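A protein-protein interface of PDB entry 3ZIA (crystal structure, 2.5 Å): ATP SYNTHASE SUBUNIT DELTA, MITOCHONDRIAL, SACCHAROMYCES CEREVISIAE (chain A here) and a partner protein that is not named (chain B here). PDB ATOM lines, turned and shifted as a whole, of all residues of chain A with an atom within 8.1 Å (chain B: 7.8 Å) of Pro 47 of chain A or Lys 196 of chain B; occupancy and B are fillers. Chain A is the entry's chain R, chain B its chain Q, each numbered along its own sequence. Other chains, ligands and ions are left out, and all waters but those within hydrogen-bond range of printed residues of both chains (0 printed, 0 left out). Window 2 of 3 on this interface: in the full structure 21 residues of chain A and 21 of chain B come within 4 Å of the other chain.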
ATOM      1  N   ASN A  44      14.704  -8.079  10.929  1.00  0.00           N
ATOM      2  CA  ASN A  44      13.252  -8.252  10.790  1.00  0.00           C
ATOM      3  C   ASN A  44      12.822  -9.714  10.720  1.00  0.00           C
ATOM      4  O   ASN A  44      12.302 -10.176   9.699  1.00  0.00           O
ATOM      5  CB  ASN A  44      12.720  -7.479   9.573  1.00  0.00           C
ATOM      6  CG  ASN A  44      12.195  -6.100   9.940  1.00  0.00           C
ATOM      7  OD1 ASN A  44      11.461  -5.939  10.916  1.00  0.00           O
ATOM      8  ND2 ASN A  44      12.562  -5.099   9.148  1.00  0.00           N
ATOM      9  N   HIS A  45      13.039 -10.434  11.819  1.00  0.00           N
ATOM     10  CA  HIS A  45      12.710 -11.856  11.896  1.00  0.00           C
ATOM     11  C   HIS A  45      11.207 -12.072  12.078  1.00  0.00           C
ATOM     12  O   HIS A  45      10.508 -11.222  12.642  1.00  0.00           O
ATOM     13  CB  HIS A  45      13.496 -12.530  13.030  1.00  0.00           C
ATOM     14  CG  HIS A  45      13.688 -14.007  12.848  1.00  0.00           C
ATOM     15  ND1 HIS A  45      14.801 -14.544  12.235  1.00  0.00           N
ATOM     16  CD2 HIS A  45      12.915 -15.060  13.207  1.00  0.00           C
ATOM     17  CE1 HIS A  45      14.702 -15.861  12.220  1.00  0.00           C
ATOM     18  NE2 HIS A  45      13.567 -16.200  12.803  1.00  0.00           N
ATOM     19  N   VAL A  46      10.728 -13.209  11.574  1.00  0.00           N
ATOM     20  CA  VAL A  46       9.339 -13.644  11.731  1.00  0.00           C
ATOM     21  C   VAL A  46       9.056 -13.895  13.216  1.00  0.00           C
ATOM     22  O   VAL A  46       9.850 -14.565  13.883  1.00  0.00           O
ATOM     23  CB  VAL A  46       9.061 -14.946  10.918  1.00  0.00           C
ATOM     24  CG1 VAL A  46       7.619 -15.433  11.111  1.00  0.00           C
ATOM     25  CG2 VAL A  46       9.366 -14.740   9.435  1.00  0.00           C
ATOM     26  N   PRO A  47       7.938 -13.343  13.741  1.00  0.00           N
ATOM     27  CA  PRO A  47       7.525 -13.642  15.114  1.00  0.00           C
ATOM     28  C   PRO A  47       7.552 -15.150  15.401  1.00  0.00           C
ATOM     29  O   PRO A  47       6.769 -15.910  14.823  1.00  0.00           O
ATOM     30  CB  PRO A  47       6.097 -13.094  15.168  1.00  0.00           C
ATOM     31  CG  PRO A  47       6.112 -11.949  14.223  1.00  0.00           C
ATOM     32  CD  PRO A  47       7.066 -12.325  13.119  1.00  0.00           C
ATOM     33  N   THR A  48       8.477 -15.562  16.268  1.00  0.00           N
ATOM     34  CA  THR A  48       8.691 -16.971  16.611  1.00  0.00           C
ATOM     35  C   THR A  48       8.868 -17.112  18.124  1.00  0.00           C
ATOM     36  O   THR A  48       9.499 -16.265  18.762  1.00  0.00           O
ATOM     37  CB  THR A  48       9.946 -17.554  15.891  1.00  0.00           C
ATOM     38  OG1 THR A  48       9.909 -17.225  14.495  1.00  0.00           O
ATOM     39  CG2 THR A  48      10.027 -19.075  16.047  1.00  0.00           C
ATOM     40  N   VAL A  49       8.294 -18.172  18.694  1.00  0.00           N
ATOM     41  CA  VAL A  49       8.493 -18.500  20.108  1.00  0.00           C
ATOM     42  C   VAL A  49       8.823 -19.983  20.279  1.00  0.00           C
ATOM     43  O   VAL A  49       7.975 -20.853  20.045  1.00  0.00           O
ATOM     44  CB  VAL A  49       7.270 -18.115  20.985  1.00  0.00           C
ATOM     45  CG1 VAL A  49       7.448 -18.621  22.414  1.00  0.00           C
ATOM     46  CG2 VAL A  49       7.061 -16.609  20.988  1.00  0.00           C
ATOM     47  N   GLU A  50      10.064 -20.253  20.683  1.00  0.00           N
ATOM     48  CA  GLU A  50      10.541 -21.621  20.904  1.00  0.00           C
ATOM     49  C   GLU A  50      11.577 -21.721  22.027  1.00  0.00           C
ATOM     50  O   GLU A  50      12.199 -20.725  22.413  1.00  0.00           O
ATOM     51  CB  GLU A  50      11.085 -22.235  19.604  1.00  0.00           C
ATOM     52  CG  GLU A  50      12.265 -21.496  18.972  1.00  0.00           C
ATOM     53  CD  GLU A  50      12.727 -22.138  17.676  1.00  0.00           C
ATOM     54  OE1 GLU A  50      12.974 -23.363  17.671  1.00  0.00           O
ATOM     55  OE2 GLU A  50      12.850 -21.416  16.663  1.00  0.00           O
ATOM     56  N   THR A  76      11.947 -15.505  22.617  1.00  0.00           N
ATOM     57  CA  THR A  76      10.713 -14.848  22.198  1.00  0.00           C
ATOM     58  C   THR A  76      11.005 -13.739  21.189  1.00  0.00           C
ATOM     59  O   THR A  76      11.730 -12.788  21.491  1.00  0.00           O
ATOM     60  CB  THR A  76       9.937 -14.265  23.405  1.00  0.00           C
ATOM     61  OG1 THR A  76       9.886 -15.231  24.463  1.00  0.00           O
ATOM     62  CG2 THR A  76       8.517 -13.880  23.005  1.00  0.00           C
ATOM     63  N   VAL A  77      10.446 -13.882  19.987  1.00  0.00           N
ATOM     64  CA  VAL A  77      10.501 -12.835  18.966  1.00  0.00           C
ATOM     65  C   VAL A  77       9.152 -12.125  18.943  1.00  0.00           C
ATOM     66  O   VAL A  77       8.110 -12.766  18.779  1.00  0.00           O
ATOM     67  CB  VAL A  77      10.835 -13.394  17.556  1.00  0.00           C
ATOM     68  CG1 VAL A  77      10.975 -12.257  16.541  1.00  0.00           C
ATOM     69  CG2 VAL A  77      12.104 -14.240  17.591  1.00  0.00           C
ATOM     70  N   GLN A  78       9.180 -10.807  19.118  1.00  0.00           N
ATOM     71  CA  GLN A  78       7.961 -10.008  19.220  1.00  0.00           C
ATOM     72  C   GLN A  78       7.600  -9.340  17.886  1.00  0.00           C
ATOM     73  O   GLN A  78       8.485  -9.110  17.053  1.00  0.00           O
ATOM     74  CB  GLN A  78       8.094  -8.968  20.344  1.00  0.00           C
ATOM     75  CG  GLN A  78       8.364  -9.560  21.742  1.00  0.00           C
ATOM     76  CD  GLN A  78       7.166 -10.290  22.363  1.00  0.00           C
ATOM     77  OE1 GLN A  78       6.107 -10.432  21.748  1.00  0.00           O
ATOM     78  NE2 GLN A  78       7.340 -10.752  23.597  1.00  0.00           N
ATOM     79  N   PRO A  79       6.294  -9.040  17.675  1.00  0.00           N
ATOM     80  CA  PRO A  79       5.827  -8.391  16.446  1.00  0.00           C
ATOM     81  C   PRO A  79       6.602  -7.122  16.085  1.00  0.00           C
ATOM     82  O   PRO A  79       6.872  -6.888  14.906  1.00  0.00           O
ATOM     83  CB  PRO A  79       4.369  -8.046  16.771  1.00  0.00           C
ATOM     84  CG  PRO A  79       3.948  -9.092  17.720  1.00  0.00           C
ATOM     85  CD  PRO A  79       5.163  -9.378  18.564  1.00  0.00           C
ATOM     86  N   ASP A  80       6.965  -6.327  17.091  1.00  0.00           N
ATOM     87  CA  ASP A  80       7.628  -5.038  16.869  1.00  0.00           C
ATOM     88  C   ASP A  80       9.169  -5.106  16.863  1.00  0.00           C
ATOM     89  O   ASP A  80       9.838  -4.267  17.481  1.00  0.00           O
ATOM     90  CB  ASP A  80       7.115  -3.990  17.877  1.00  0.00           C
ATOM     91  CG  ASP A  80       7.293  -4.421  19.336  1.00  0.00           C
ATOM     92  OD1 ASP A  80       7.656  -5.592  19.603  1.00  0.00           O
ATOM     93  OD2 ASP A  80       7.064  -3.574  20.223  1.00  0.00           O
ATOM     94  N   SER A  81       9.720  -6.096  16.151  1.00  0.00           N
ATOM     95  CA  SER A  81      11.181  -6.281  15.993  1.00  0.00           C
ATOM     96  C   SER A  81      11.968  -6.327  17.316  1.00  0.00           C
ATOM     97  O   SER A  81      13.039  -5.718  17.438  1.00  0.00           O
ATOM     98  CB  SER A  81      11.774  -5.222  15.046  1.00  0.00           C
ATOM     99  OG  SER A  81      11.407  -5.463  13.700  1.00  0.00           O
ATOM    100  N   GLN A  82      11.427  -7.056  18.293  1.00  0.00           N
ATOM    101  CA  GLN A  82      12.050  -7.195  19.612  1.00  0.00           C
ATOM    102  C   GLN A  82      12.364  -8.647  19.926  1.00  0.00           C
ATOM    103  O   GLN A  82      11.562  -9.541  19.648  1.00  0.00           O
ATOM    104  CB  GLN A  82      11.147  -6.625  20.708  1.00  0.00           C
ATOM    105  CG  GLN A  82      11.255  -5.120  20.895  1.00  0.00           C
ATOM    106  CD  GLN A  82      10.180  -4.557  21.813  1.00  0.00           C
ATOM    107  OE1 GLN A  82       9.575  -5.282  22.608  1.00  0.00           O
ATOM    108  NE2 GLN A  82       9.937  -3.253  21.704  1.00  0.00           N
ATOM    109  N   PHE B  51       4.754 -12.266  26.140  1.00  0.00           N
ATOM    110  CA  PHE B  51       4.037 -13.252  25.339  1.00  0.00           C
ATOM    111  C   PHE B  51       2.557 -13.301  25.728  1.00  0.00           C
ATOM    112  O   PHE B  51       1.692 -13.402  24.861  1.00  0.00           O
ATOM    113  CB  PHE B  51       4.678 -14.637  25.493  1.00  0.00           C
ATOM    114  CG  PHE B  51       3.763 -15.778  25.126  1.00  0.00           C
ATOM    115  CD1 PHE B  51       3.649 -16.202  23.804  1.00  0.00           C
ATOM    116  CD2 PHE B  51       3.010 -16.427  26.105  1.00  0.00           C
ATOM    117  CE1 PHE B  51       2.799 -17.254  23.461  1.00  0.00           C
ATOM    118  CE2 PHE B  51       2.156 -17.477  25.772  1.00  0.00           C
ATOM    119  CZ  PHE B  51       2.053 -17.894  24.449  1.00  0.00           C
ATOM    120  N   ASN B  54       0.453 -10.093  24.364  1.00  0.00           N
ATOM    121  CA  ASN B  54       0.068 -10.234  22.960  1.00  0.00           C
ATOM    122  C   ASN B  54      -0.897 -11.394  22.721  1.00  0.00           C
ATOM    123  O   ASN B  54      -1.940 -11.208  22.089  1.00  0.00           O
ATOM    124  CB  ASN B  54       1.312 -10.374  22.073  1.00  0.00           C
ATOM    125  CG  ASN B  54       2.129  -9.093  21.999  1.00  0.00           C
ATOM    126  OD1 ASN B  54       1.626  -8.039  21.610  1.00  0.00           O
ATOM    127  ND2 ASN B  54       3.400  -9.184  22.363  1.00  0.00           N
ATOM    128  N   ALA B  55      -0.552 -12.577  23.235  1.00  0.00           N
ATOM    129  CA  ALA B  55      -1.416 -13.762  23.139  1.00  0.00           C
ATOM    130  C   ALA B  55      -2.715 -13.592  23.927  1.00  0.00           C
ATOM    131  O   ALA B  55      -3.689 -14.310  23.682  1.00  0.00           O
ATOM    132  CB  ALA B  55      -0.676 -15.013  23.586  1.00  0.00           C
ATOM    133  N   GLU B  56      -2.710 -12.647  24.872  1.00  0.00           N
ATOM    134  CA  GLU B  56      -3.925 -12.155  25.533  1.00  0.00           C
ATOM    135  C   GLU B  56      -4.675 -13.275  26.271  1.00  0.00           C
ATOM    136  O   GLU B  56      -5.856 -13.526  26.014  1.00  0.00           O
ATOM    137  CB  GLU B  56      -4.824 -11.466  24.495  1.00  0.00           C
ATOM    138  CG  GLU B  56      -5.726 -10.360  25.024  1.00  0.00           C
ATOM    139  CD  GLU B  56      -6.515  -9.671  23.914  1.00  0.00           C
ATOM    140  OE1 GLU B  56      -6.593 -10.223  22.791  1.00  0.00           O
ATOM    141  OE2 GLU B  56      -7.059  -8.575  24.167  1.00  0.00           O
ATOM    142  N   SER B 191      -5.551 -19.219  24.071  1.00  0.00           N
ATOM    143  CA  SER B 191      -5.393 -17.760  24.046  1.00  0.00           C
ATOM    144  C   SER B 191      -5.686 -17.198  22.645  1.00  0.00           C
ATOM    145  O   SER B 191      -5.193 -17.734  21.647  1.00  0.00           O
ATOM    146  CB  SER B 191      -4.003 -17.333  24.551  1.00  0.00           C
ATOM    147  OG  SER B 191      -2.972 -18.180  24.076  1.00  0.00           O
ATOM    148  N   PRO B 192      -6.522 -16.137  22.573  1.00  0.00           N
ATOM    149  CA  PRO B 192      -7.018 -15.502  21.339  1.00  0.00           C
ATOM    150  C   PRO B 192      -5.993 -15.259  20.220  1.00  0.00           C
ATOM    151  O   PRO B 192      -6.284 -15.556  19.060  1.00  0.00           O
ATOM    152  CB  PRO B 192      -7.585 -14.174  21.848  1.00  0.00           C
ATOM    153  CG  PRO B 192      -8.118 -14.516  23.193  1.00  0.00           C
ATOM    154  CD  PRO B 192      -7.193 -15.574  23.763  1.00  0.00           C
ATOM    155  N   SER B 193      -4.822 -14.727  20.561  1.00  0.00           N
ATOM    156  CA  SER B 193      -3.790 -14.428  19.560  1.00  0.00           C
ATOM    157  C   SER B 193      -2.623 -15.422  19.581  1.00  0.00           C
ATOM    158  O   SER B 193      -1.559 -15.154  19.013  1.00  0.00           O
ATOM    159  CB  SER B 193      -3.282 -12.992  19.722  1.00  0.00           C
ATOM    160  OG  SER B 193      -4.250 -12.048  19.298  1.00  0.00           O
ATOM    161  N   PHE B 194      -2.846 -16.571  20.224  1.00  0.00           N
ATOM    162  CA  PHE B 194      -1.839 -17.627  20.408  1.00  0.00           C
ATOM    163  C   PHE B 194      -1.041 -17.998  19.151  1.00  0.00           C
ATOM    164  O   PHE B 194       0.184 -18.140  19.211  1.00  0.00           O
ATOM    165  CB  PHE B 194      -2.505 -18.876  21.008  1.00  0.00           C
ATOM    166  CG  PHE B 194      -1.655 -20.122  20.955  1.00  0.00           C
ATOM    167  CD1 PHE B 194      -0.473 -20.218  21.694  1.00  0.00           C
ATOM    168  CD2 PHE B 194      -2.054 -21.213  20.183  1.00  0.00           C
ATOM    169  CE1 PHE B 194       0.309 -21.375  21.649  1.00  0.00           C
ATOM    170  CE2 PHE B 194      -1.282 -22.378  20.134  1.00  0.00           C
ATOM    171  CZ  PHE B 194      -0.096 -22.459  20.869  1.00  0.00           C
ATOM    172  N   GLY B 195      -1.742 -18.148  18.028  1.00  0.00           N
ATOM    173  CA  GLY B 195      -1.142 -18.626  16.781  1.00  0.00           C
ATOM    174  C   GLY B 195      -0.302 -17.642  15.980  1.00  0.00           C
ATOM    175  O   GLY B 195       0.305 -18.027  14.978  1.00  0.00           O
ATOM    176  N   LYS B 196      -0.250 -16.382  16.416  1.00  0.00           N
ATOM    177  CA  LYS B 196       0.505 -15.330  15.708  1.00  0.00           C
ATOM    178  C   LYS B 196       2.021 -15.568  15.630  1.00  0.00           C
ATOM    179  O   LYS B 196       2.728 -14.898  14.868  1.00  0.00           O
ATOM    180  CB  LYS B 196       0.221 -13.950  16.313  1.00  0.00           C
ATOM    181  CG  LYS B 196      -1.091 -13.335  15.848  1.00  0.00           C
ATOM    182  CD  LYS B 196      -1.059 -11.810  15.891  1.00  0.00           C
ATOM    183  CE  LYS B 196      -1.412 -11.270  17.269  1.00  0.00           C
ATOM    184  NZ  LYS B 196      -1.604  -9.796  17.250  1.00  0.00           N
ATOM    185  N   PHE B 197       2.507 -16.521  16.423  1.00  0.00           N
ATOM    186  CA  PHE B 197       3.921 -16.880  16.451  1.00  0.00           C
ATOM    187  C   PHE B 197       4.110 -18.276  15.876  1.00  0.00           C
ATOM    188  O   PHE B 197       3.305 -19.174  16.141  1.00  0.00           O
ATOM    189  CB  PHE B 197       4.466 -16.814  17.886  1.00  0.00           C
ATOM    190  CG  PHE B 197       4.294 -15.465  18.546  1.00  0.00           C
ATOM    191  CD1 PHE B 197       5.256 -14.465  18.387  1.00  0.00           C
ATOM    192  CD2 PHE B 197       3.169 -15.194  19.324  1.00  0.00           C
ATOM    193  CE1 PHE B 197       5.097 -13.212  18.987  1.00  0.00           C
ATOM    194  CE2 PHE B 197       3.002 -13.943  19.930  1.00  0.00           C
ATOM    195  CZ  PHE B 197       3.971 -12.952  19.761  1.00  0.00           C
ATOM    196  N   GLU B 198       5.164 -18.450  15.081  1.00  0.00           N
ATOM    197  CA  GLU B 198       5.495 -19.762  14.527  1.00  0.00           C
ATOM    198  C   GLU B 198       5.839 -20.726  15.661  1.00  0.00           C
ATOM    199  O   GLU B 198       6.814 -20.526  16.395  1.00  0.00           O
ATOM    200  CB  GLU B 198       6.635 -19.668  13.498  1.00  0.00           C
ATOM    201  CG  GLU B 198       7.022 -21.000  12.827  1.00  0.00           C
ATOM    202  CD  GLU B 198       5.917 -21.611  11.957  1.00  0.00           C
ATOM    203  OE1 GLU B 198       4.875 -20.958  11.727  1.00  0.00           O
ATOM    204  OE2 GLU B 198       6.100 -22.758  11.496  1.00  0.00           O
ATOM    205  N   ILE B 199       5.009 -21.757  15.809  1.00  0.00           N
ATOM    206  CA  ILE B 199       5.134 -22.703  16.912  1.00  0.00           C
ATOM    207  C   ILE B 199       5.063 -24.136  16.400  1.00  0.00           C
ATOM    208  O   ILE B 199       4.167 -24.488  15.626  1.00  0.00           O
ATOM    209  CB  ILE B 199       4.040 -22.467  17.997  1.00  0.00           C
ATOM    210  CG1 ILE B 199       4.169 -21.065  18.601  1.00  0.00           C
ATOM    211  CG2 ILE B 199       4.141 -23.507  19.110  1.00  0.00           C
ATOM    212  CD1 ILE B 199       2.909 -20.556  19.265  1.00  0.00           C
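Hydrophobic or aromatic side chains of chain A within 4 Å of the printed part of chain B: Pro 47, Val 49 and Pro 79. Among the printed residues, 11 pairs touch across the chains.
ND2 of Asn 54 of chain B is in hydrogen-bond range of OE1 of Gln 78 of chain A. The backbone carbonyl oxygen of Pro 47 of chain A sits at hydrogen-bond distance from the backbone NH of Glu 198 of chain B (3.0 Å).
Of the printed residues of chain B, Thr 48 of chain A touches Glu 198. Of the printed residues of chain B, Val 77 of chain A touches Phe 197 (3.1 Å). Of the printed residues of chain B, Pro 79 of chain A touches Phe 197. Asp 80 of chain A touches none of the printed residues of chain B. Gly 195 of chain B touches none of the printed residues of chain A. Of the printed residues of chain A, Lys 196 of chain B touches Pro 47. Printed residues of chain A within 4 Å of Phe 197 of chain B: Pro 47 (3.4 Å), Val 49 (3.8 Å), Val 77 (3.1 Å), Gln 78 (3.9 Å) and Pro 79 (3.9 Å). The nearest residue of chain B that does not touch Pro 47 of chain A is Ile 199 of chain B (6.2 Å).
Pro 47 of chain A touches Lys 196 of chain B. CA of Phe 197 of chain B touches O of Pro 47 of chain A, at 3.4 Å. CG2 of Thr 48 of chain A touches O of Glu 198 of chain B (3.5 Å). Val 49 of chain A touches Phe 197 of chain B. Glu 198 of chain B touches Val 49 of chain A. Phe 197 of chain B touches Val 77 of chain A. Phe 51 of chain B touches Gln 78 of chain A. Gln 78 of chain A touches Phe 197 of chain B. Phe 197 of chain B touches Pro 79 of chain A (CE1 to CD, 3.9 Å).
OG1 of Thr 48 of chain A sits at hydrogen-bond distance from O of Val 46 of chain A, 2.7 Å away. N of Val 77 of chain A is in hydrogen-bond range of O of Thr 48 of chain A (2.8 Å).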
